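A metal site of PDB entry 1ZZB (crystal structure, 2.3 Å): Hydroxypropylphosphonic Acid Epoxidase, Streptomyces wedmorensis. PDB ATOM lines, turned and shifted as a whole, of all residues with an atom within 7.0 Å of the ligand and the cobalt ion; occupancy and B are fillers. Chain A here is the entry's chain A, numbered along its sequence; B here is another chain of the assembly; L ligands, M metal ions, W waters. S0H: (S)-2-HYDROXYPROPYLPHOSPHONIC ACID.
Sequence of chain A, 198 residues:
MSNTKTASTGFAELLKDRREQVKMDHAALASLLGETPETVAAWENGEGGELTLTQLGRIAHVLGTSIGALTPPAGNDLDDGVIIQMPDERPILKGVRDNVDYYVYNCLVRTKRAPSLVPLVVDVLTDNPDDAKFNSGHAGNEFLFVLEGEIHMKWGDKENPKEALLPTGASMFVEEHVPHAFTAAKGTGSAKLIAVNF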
ATOM      1  N   TYR A 102     -20.046  17.312 -21.852  1.00  0.00           N
ATOM      2  CA  TYR A 102     -20.082  16.289 -22.895  1.00  0.00           C
ATOM      3  C   TYR A 102     -20.612  16.759 -24.250  1.00  0.00           C
ATOM      4  O   TYR A 102     -20.006  16.470 -25.286  1.00  0.00           O
ATOM      5  CB  TYR A 102     -20.909  15.106 -22.407  1.00  0.00           C
ATOM      6  CG  TYR A 102     -20.568  13.777 -23.060  1.00  0.00           C
ATOM      7  CD1 TYR A 102     -19.322  13.177 -22.869  1.00  0.00           C
ATOM      8  CD2 TYR A 102     -21.509  13.114 -23.848  1.00  0.00           C
ATOM      9  CE1 TYR A 102     -19.024  11.944 -23.440  1.00  0.00           C
ATOM     10  CE2 TYR A 102     -21.209  11.873 -24.426  1.00  0.00           C
ATOM     11  CZ  TYR A 102     -19.977  11.297 -24.220  1.00  0.00           C
ATOM     12  OH  TYR A 102     -19.698  10.060 -24.777  1.00  0.00           O
ATOM     13  N   TYR A 103     -21.756  17.452 -24.242  1.00  0.00           N
ATOM     14  CA  TYR A 103     -22.364  17.958 -25.471  1.00  0.00           C
ATOM     15  C   TYR A 103     -22.780  19.430 -25.380  1.00  0.00           C
ATOM     16  O   TYR A 103     -22.768  20.060 -24.321  1.00  0.00           O
ATOM     17  CB  TYR A 103     -23.659  17.198 -25.799  1.00  0.00           C
ATOM     18  CG  TYR A 103     -23.559  15.713 -26.081  1.00  0.00           C
ATOM     19  CD1 TYR A 103     -24.675  14.896 -25.908  1.00  0.00           C
ATOM     20  CD2 TYR A 103     -22.378  15.126 -26.529  1.00  0.00           C
ATOM     21  CE1 TYR A 103     -24.616  13.529 -26.149  1.00  0.00           C
ATOM     22  CE2 TYR A 103     -22.316  13.743 -26.784  1.00  0.00           C
ATOM     23  CZ  TYR A 103     -23.439  12.963 -26.578  1.00  0.00           C
ATOM     24  OH  TYR A 103     -23.401  11.592 -26.758  1.00  0.00           O
ATOM     25  N   TYR A 105     -26.075  21.266 -27.113  1.00  0.00           N
ATOM     26  CA  TYR A 105     -27.272  21.103 -27.929  1.00  0.00           C
ATOM     27  C   TYR A 105     -27.733  22.411 -28.545  1.00  0.00           C
ATOM     28  O   TYR A 105     -28.007  23.385 -27.836  1.00  0.00           O
ATOM     29  CB  TYR A 105     -28.421  20.546 -27.101  1.00  0.00           C
ATOM     30  CG  TYR A 105     -28.124  19.243 -26.407  1.00  0.00           C
ATOM     31  CD1 TYR A 105     -27.912  19.215 -25.026  1.00  0.00           C
ATOM     32  CD2 TYR A 105     -28.082  18.042 -27.112  1.00  0.00           C
ATOM     33  CE1 TYR A 105     -27.673  18.003 -24.359  1.00  0.00           C
ATOM     34  CE2 TYR A 105     -27.845  16.831 -26.463  1.00  0.00           C
ATOM     35  CZ  TYR A 105     -27.639  16.819 -25.086  1.00  0.00           C
ATOM     36  OH  TYR A 105     -27.434  15.636 -24.431  1.00  0.00           O
ATOM     37  N   LEU A 120     -31.964  18.352 -33.292  1.00  0.00           N
ATOM     38  CA  LEU A 120     -30.836  19.080 -32.735  1.00  0.00           C
ATOM     39  C   LEU A 120     -29.597  18.990 -33.609  1.00  0.00           C
ATOM     40  O   LEU A 120     -29.480  18.122 -34.482  1.00  0.00           O
ATOM     41  CB  LEU A 120     -30.461  18.491 -31.373  1.00  0.00           C
ATOM     42  CG  LEU A 120     -31.559  18.146 -30.375  1.00  0.00           C
ATOM     43  CD1 LEU A 120     -30.997  17.181 -29.339  1.00  0.00           C
ATOM     44  CD2 LEU A 120     -32.081  19.418 -29.703  1.00  0.00           C
ATOM     45  N   VAL A 122     -25.927  18.557 -32.595  1.00  0.00           N
ATOM     46  CA  VAL A 122     -25.149  18.290 -31.399  1.00  0.00           C
ATOM     47  C   VAL A 122     -23.654  18.380 -31.639  1.00  0.00           C
ATOM     48  O   VAL A 122     -23.124  17.846 -32.627  1.00  0.00           O
ATOM     49  CB  VAL A 122     -25.460  16.883 -30.831  1.00  0.00           C
ATOM     50  CG1 VAL A 122     -24.746  16.686 -29.500  1.00  0.00           C
ATOM     51  CG2 VAL A 122     -26.957  16.702 -30.670  1.00  0.00           C
ATOM     52  N   LYS A 133     -19.820   8.425 -21.914  1.00  0.00           N
ATOM     53  CA  LYS A 133     -20.830   8.286 -20.869  1.00  0.00           C
ATOM     54  C   LYS A 133     -22.209   8.036 -21.472  1.00  0.00           C
ATOM     55  O   LYS A 133     -22.842   8.946 -22.026  1.00  0.00           O
ATOM     56  CB  LYS A 133     -20.858   9.540 -19.988  1.00  0.00           C
ATOM     57  N   PHE A 134     -22.667   6.787 -21.360  1.00  0.00           N
ATOM     58  CA  PHE A 134     -23.967   6.376 -21.895  1.00  0.00           C
ATOM     59  C   PHE A 134     -25.109   7.083 -21.203  1.00  0.00           C
ATOM     60  O   PHE A 134     -24.972   7.535 -20.059  1.00  0.00           O
ATOM     61  CB  PHE A 134     -24.171   4.878 -21.692  1.00  0.00           C
ATOM     62  CG  PHE A 134     -23.396   4.011 -22.650  1.00  0.00           C
ATOM     63  CD1 PHE A 134     -22.002   4.047 -22.666  1.00  0.00           C
ATOM     64  CD2 PHE A 134     -24.061   3.147 -23.507  1.00  0.00           C
ATOM     65  CE1 PHE A 134     -21.287   3.199 -23.520  1.00  0.00           C
ATOM     66  CE2 PHE A 134     -23.354   2.300 -24.365  1.00  0.00           C
ATOM     67  CZ  PHE A 134     -21.956   2.328 -24.370  1.00  0.00           C
ATOM     68  N   ASN A 135     -26.239   7.195 -21.900  1.00  0.00           N
ATOM     69  CA  ASN A 135     -27.437   7.763 -21.292  1.00  0.00           C
ATOM     70  C   ASN A 135     -28.170   6.488 -20.893  1.00  0.00           C
ATOM     71  O   ASN A 135     -27.766   5.405 -21.317  1.00  0.00           O
ATOM     72  CB  ASN A 135     -28.267   8.595 -22.304  1.00  0.00           C
ATOM     73  CG  ASN A 135     -28.707   7.788 -23.515  1.00  0.00           C
ATOM     74  OD1 ASN A 135     -29.145   6.642 -23.378  1.00  0.00           O
ATOM     75  ND2 ASN A 135     -28.612   8.393 -24.698  1.00  0.00           N
ATOM     76  N   SER A 136     -29.215   6.575 -20.090  1.00  0.00           N
ATOM     77  CA  SER A 136     -29.923   5.367 -19.668  1.00  0.00           C
ATOM     78  C   SER A 136     -30.913   4.890 -20.733  1.00  0.00           C
ATOM     79  O   SER A 136     -31.679   3.949 -20.513  1.00  0.00           O
ATOM     80  CB  SER A 136     -30.636   5.625 -18.342  1.00  0.00           C
ATOM     81  N   GLY A 137     -30.864   5.526 -21.901  1.00  0.00           N
ATOM     82  CA  GLY A 137     -31.788   5.187 -22.970  1.00  0.00           C
ATOM     83  C   GLY A 137     -32.964   6.138 -22.836  1.00  0.00           C
ATOM     84  O   GLY A 137     -33.283   6.569 -21.722  1.00  0.00           O
ATOM     85  N   HIS A 138     -33.613   6.485 -23.937  1.00  0.00           N
ATOM     86  CA  HIS A 138     -34.750   7.392 -23.851  1.00  0.00           C
ATOM     87  C   HIS A 138     -35.888   7.002 -24.790  1.00  0.00           C
ATOM     88  O   HIS A 138     -35.676   6.354 -25.803  1.00  0.00           O
ATOM     89  CB  HIS A 138     -34.306   8.841 -24.123  1.00  0.00           C
ATOM     90  CG  HIS A 138     -33.556   9.030 -25.401  1.00  0.00           C
ATOM     91  ND1 HIS A 138     -34.121   8.805 -26.638  1.00  0.00           N
ATOM     92  CD2 HIS A 138     -32.286   9.447 -25.645  1.00  0.00           C
ATOM     93  CE1 HIS A 138     -33.233   9.078 -27.589  1.00  0.00           C
ATOM     94  NE2 HIS A 138     -32.122   9.462 -27.009  1.00  0.00           N
ATOM     95  N   GLU A 142     -34.579   7.652 -32.749  1.00  0.00           N
ATOM     96  CA  GLU A 142     -33.671   8.737 -33.055  1.00  0.00           C
ATOM     97  C   GLU A 142     -32.849   8.536 -34.326  1.00  0.00           C
ATOM     98  O   GLU A 142     -32.084   7.583 -34.438  1.00  0.00           O
ATOM     99  CB  GLU A 142     -32.730   8.986 -31.875  1.00  0.00           C
ATOM    100  CG  GLU A 142     -31.767  10.153 -32.075  1.00  0.00           C
ATOM    101  CD  GLU A 142     -30.982  10.497 -30.814  1.00  0.00           C
ATOM    102  OE1 GLU A 142     -30.096  11.390 -30.885  1.00  0.00           O
ATOM    103  OE2 GLU A 142     -31.246   9.892 -29.752  1.00  0.00           O
ATOM    104  N   LEU A 144     -29.927   9.932 -36.855  1.00  0.00           N
ATOM    105  CA  LEU A 144     -28.745  10.769 -36.723  1.00  0.00           C
ATOM    106  C   LEU A 144     -28.000  10.843 -38.040  1.00  0.00           C
ATOM    107  O   LEU A 144     -28.151   9.973 -38.901  1.00  0.00           O
ATOM    108  CB  LEU A 144     -27.818  10.248 -35.614  1.00  0.00           C
ATOM    109  CG  LEU A 144     -28.320  10.374 -34.174  1.00  0.00           C
ATOM    110  CD1 LEU A 144     -29.148   9.163 -33.810  1.00  0.00           C
ATOM    111  CD2 LEU A 144     -27.135  10.473 -33.225  1.00  0.00           C
ATOM    112  N   VAL A 174     -31.316   4.739 -33.880  1.00  0.00           N
ATOM    113  CA  VAL A 174     -31.283   3.976 -32.637  1.00  0.00           C
ATOM    114  C   VAL A 174     -32.712   3.900 -32.114  1.00  0.00           C
ATOM    115  O   VAL A 174     -33.385   4.912 -31.909  1.00  0.00           O
ATOM    116  CB  VAL A 174     -30.284   4.582 -31.580  1.00  0.00           C
ATOM    117  CG1 VAL A 174     -29.535   5.754 -32.167  1.00  0.00           C
ATOM    118  CG2 VAL A 174     -31.009   4.944 -30.300  1.00  0.00           C
ATOM    119  N   VAL A 178     -33.039   2.214 -26.298  1.00  0.00           N
ATOM    120  CA  VAL A 178     -31.717   1.631 -26.434  1.00  0.00           C
ATOM    121  C   VAL A 178     -30.692   2.655 -25.954  1.00  0.00           C
ATOM    122  O   VAL A 178     -30.558   3.731 -26.538  1.00  0.00           O
ATOM    123  CB  VAL A 178     -31.389   1.273 -27.898  1.00  0.00           C
ATOM    124  CG1 VAL A 178     -29.945   0.815 -27.995  1.00  0.00           C
ATOM    125  CG2 VAL A 178     -32.325   0.180 -28.401  1.00  0.00           C
ATOM    126  N   HIS A 180     -27.315   4.736 -25.426  1.00  0.00           N
ATOM    127  CA  HIS A 180     -26.215   5.051 -26.326  1.00  0.00           C
ATOM    128  C   HIS A 180     -25.287   6.146 -25.828  1.00  0.00           C
ATOM    129  O   HIS A 180     -25.589   6.843 -24.863  1.00  0.00           O
ATOM    130  CB  HIS A 180     -26.756   5.451 -27.711  1.00  0.00           C
ATOM    131  CG  HIS A 180     -27.901   6.411 -27.657  1.00  0.00           C
ATOM    132  ND1 HIS A 180     -29.120   6.088 -27.089  1.00  0.00           N
ATOM    133  CD2 HIS A 180     -28.017   7.682 -28.112  1.00  0.00           C
ATOM    134  CE1 HIS A 180     -29.943   7.112 -27.217  1.00  0.00           C
ATOM    135  NE2 HIS A 180     -29.303   8.083 -27.831  1.00  0.00           N
ATOM    136  N   ALA A 181     -24.155   6.294 -26.524  1.00  0.00           N
ATOM    137  CA  ALA A 181     -23.131   7.277 -26.197  1.00  0.00           C
ATOM    138  C   ALA A 181     -22.361   7.678 -27.469  1.00  0.00           C
ATOM    139  O   ALA A 181     -22.235   6.895 -28.393  1.00  0.00           O
ATOM    140  CB  ALA A 181     -22.187   6.695 -25.169  1.00  0.00           C
ATOM    141  N   PHE A 182     -21.834   8.897 -27.482  1.00  0.00           N
ATOM    142  CA  PHE A 182     -21.093   9.390 -28.635  1.00  0.00           C
ATOM    143  C   PHE A 182     -19.878  10.217 -28.234  1.00  0.00           C
ATOM    144  O   PHE A 182     -19.899  10.905 -27.219  1.00  0.00           O
ATOM    145  CB  PHE A 182     -21.997  10.280 -29.499  1.00  0.00           C
ATOM    146  CG  PHE A 182     -23.124   9.545 -30.173  1.00  0.00           C
ATOM    147  CD1 PHE A 182     -22.893   8.764 -31.306  1.00  0.00           C
ATOM    148  CD2 PHE A 182     -24.425   9.637 -29.675  1.00  0.00           C
ATOM    149  CE1 PHE A 182     -23.925   8.075 -31.947  1.00  0.00           C
ATOM    150  CE2 PHE A 182     -25.477   8.945 -30.301  1.00  0.00           C
ATOM    151  CZ  PHE A 182     -25.226   8.167 -31.448  1.00  0.00           C
ATOM    152  N   ALA A 195     -29.123  15.249 -34.822  1.00  0.00           N
ATOM    153  CA  ALA A 195     -29.893  14.168 -34.221  1.00  0.00           C
ATOM    154  C   ALA A 195     -31.357  14.566 -34.200  1.00  0.00           C
ATOM    155  O   ALA A 195     -31.699  15.702 -33.853  1.00  0.00           O
ATOM    156  CB  ALA A 195     -29.393  13.899 -32.813  1.00  0.00           C
ATOM    157  N   ASN A 197     -35.028  13.219 -32.698  1.00  0.00           N
ATOM    158  CA  ASN A 197     -35.869  12.317 -31.904  1.00  0.00           C
ATOM    159  C   ASN A 197     -37.286  12.480 -32.437  1.00  0.00           C
ATOM    160  O   ASN A 197     -37.731  13.593 -32.713  1.00  0.00           O
ATOM    161  CB  ASN A 197     -35.830  12.707 -30.432  1.00  0.00           C
ATOM    162  CG  ASN A 197     -34.417  12.762 -29.888  1.00  0.00           C
ATOM    163  OD1 ASN A 197     -33.851  11.752 -29.469  1.00  0.00           O
ATOM    164  ND2 ASN A 197     -33.822  13.960 -29.907  1.00  0.00           N
ATOM    165  N   GLU B  20     -35.927  16.367 -19.907  1.00  0.00           N
ATOM    166  CA  GLU B  20     -34.712  15.729 -20.397  1.00  0.00           C
ATOM    167  C   GLU B  20     -34.748  15.585 -21.906  1.00  0.00           C
ATOM    168  O   GLU B  20     -33.742  15.852 -22.572  1.00  0.00           O
ATOM    169  CB  GLU B  20     -34.515  14.360 -19.713  1.00  0.00           C
ATOM    170  CG  GLU B  20     -34.081  14.487 -18.255  1.00  0.00           C
ATOM    171  CD  GLU B  20     -33.875  13.145 -17.554  1.00  0.00           C
ATOM    172  OE1 GLU B  20     -33.449  13.153 -16.380  1.00  0.00           O
ATOM    173  OE2 GLU B  20     -34.142  12.094 -18.170  1.00  0.00           O
ATOM    174  N   GLN B  21     -35.895  15.207 -22.458  1.00  0.00           N
ATOM    175  CA  GLN B  21     -35.959  15.054 -23.916  1.00  0.00           C
ATOM    176  C   GLN B  21     -35.873  16.373 -24.687  1.00  0.00           C
ATOM    177  O   GLN B  21     -35.554  16.361 -25.871  1.00  0.00           O
ATOM    178  CB  GLN B  21     -37.202  14.255 -24.341  1.00  0.00           C
ATOM    179  CG  GLN B  21     -38.432  14.452 -23.511  1.00  0.00           C
ATOM    180  CD  GLN B  21     -39.571  13.544 -23.939  1.00  0.00           C
ATOM    181  OE1 GLN B  21     -39.989  13.563 -25.096  1.00  0.00           O
ATOM    182  NE2 GLN B  21     -40.085  12.761 -22.997  1.00  0.00           N
ATOM    183  N   LYS B  23     -33.809  18.614 -23.697  1.00  0.00           N
ATOM    184  CA  LYS B  23     -32.466  19.017 -23.298  1.00  0.00           C
ATOM    185  C   LYS B  23     -32.359  20.170 -22.296  1.00  0.00           C
ATOM    186  O   LYS B  23     -31.323  20.850 -22.235  1.00  0.00           O
ATOM    187  CB  LYS B  23     -31.642  19.356 -24.546  1.00  0.00           C
ATOM    188  CG  LYS B  23     -31.750  18.306 -25.638  1.00  0.00           C
ATOM    189  CD  LYS B  23     -31.537  16.899 -25.092  1.00  0.00           C
ATOM    190  CE  LYS B  23     -31.947  15.838 -26.108  1.00  0.00           C
ATOM    191  NZ  LYS B  23     -31.804  14.453 -25.574  1.00  0.00           N
HETATM  192  P1  S0H L   1     -28.630  12.083 -25.663  1.00  0.00           P
HETATM  193  C2  S0H L   1     -27.397  11.174 -24.647  1.00  0.00           C
HETATM  194  C3  S0H L   1     -27.011  11.919 -23.331  1.00  0.00           C
HETATM  195  O6  S0H L   1     -26.015  11.221 -22.637  1.00  0.00           O
HETATM  196  C1  S0H L   1     -26.556  12.888 -23.554  1.00  0.00           C
HETATM  197  O13 S0H L   1     -29.529  12.926 -24.897  1.00  0.00           O
HETATM  198  O14 S0H L   1     -29.431  11.066 -26.517  1.00  0.00           O
HETATM  199  O15 S0H L   1     -27.902  12.809 -26.827  1.00  0.00           O
HETATM  200 CO    CO M   1     -30.290  10.116 -27.885  1.00  0.00          CO
HETATM  201  O   HOH W   1     -28.139  11.122 -28.750  1.00  0.00           O
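Water W1 bridges an oxygen (O15) of the ligand and the side-chain carboxylate of Glu 142.
Merely in contact with the ligand: Tyr 103 and Lys 133. Hydrophobic or aromatic side chains within 4 Å of the ligand: Tyr 103, His 138 and His 180. Of the 23 residues printed, 8 come within 4 Å of the ligand. Along chain A the residues within 4 Å of the ligand span positions 103 to 180.
The cobalt ion is bound by O14 of the ligand (1.9 Å), OE2 of Glu 142 (2.1 Å), NE2 of His 138 (2.1 Å), NE2 of His 180 (2.3 Å) and water W1 (2.5 Å). The cobalt ion has five donor atoms within binding distance.
Merely in contact with the cobalt ion: Asn 135 (3.99 Å). Of the 23 residues printed, 4 come within 4 Å of the cobalt ion. The nearest printed residue that does not touch the cobalt ion is Asn 197 (4.2 Å).
O13 of the ligand lies within salt-bridge range of NZ of Lys 23 of chain B (2.8 Å). The side-chain hydroxyl (OH) of Tyr 105 lies close to an oxygen (O13) of the ligand. ND2 of Asn 135 sits close to O14 of the ligand, at 3.3 Å.
OE2 of Glu 142 sits close to OD1 of Asn 197 (3.2 Å). O of Glu 142 lies within hydrogen-bond range of N of Val 174 (3.0 Å). N of Asn 135 lies within hydrogen-bond range of O of His 180, 3.1 Å away. ND1 of His 180 is in hydrogen-bond range of O of Val 178, 2.8 Å away. The side-chain amide oxygen of Asn 135 is in hydrogen-bond range of the backbone NH of Gly 137 (2.5 Å). The side-chain hydroxyl (OH) of Tyr 103 is in hydrogen-bond range of the backbone NH (N) of Phe 182, 3.2 Å away. The side-chain hydroxyl (OH) of Tyr 102 sits at hydrogen-bond distance from the backbone NH (N) of Lys 133 (3.3 Å).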
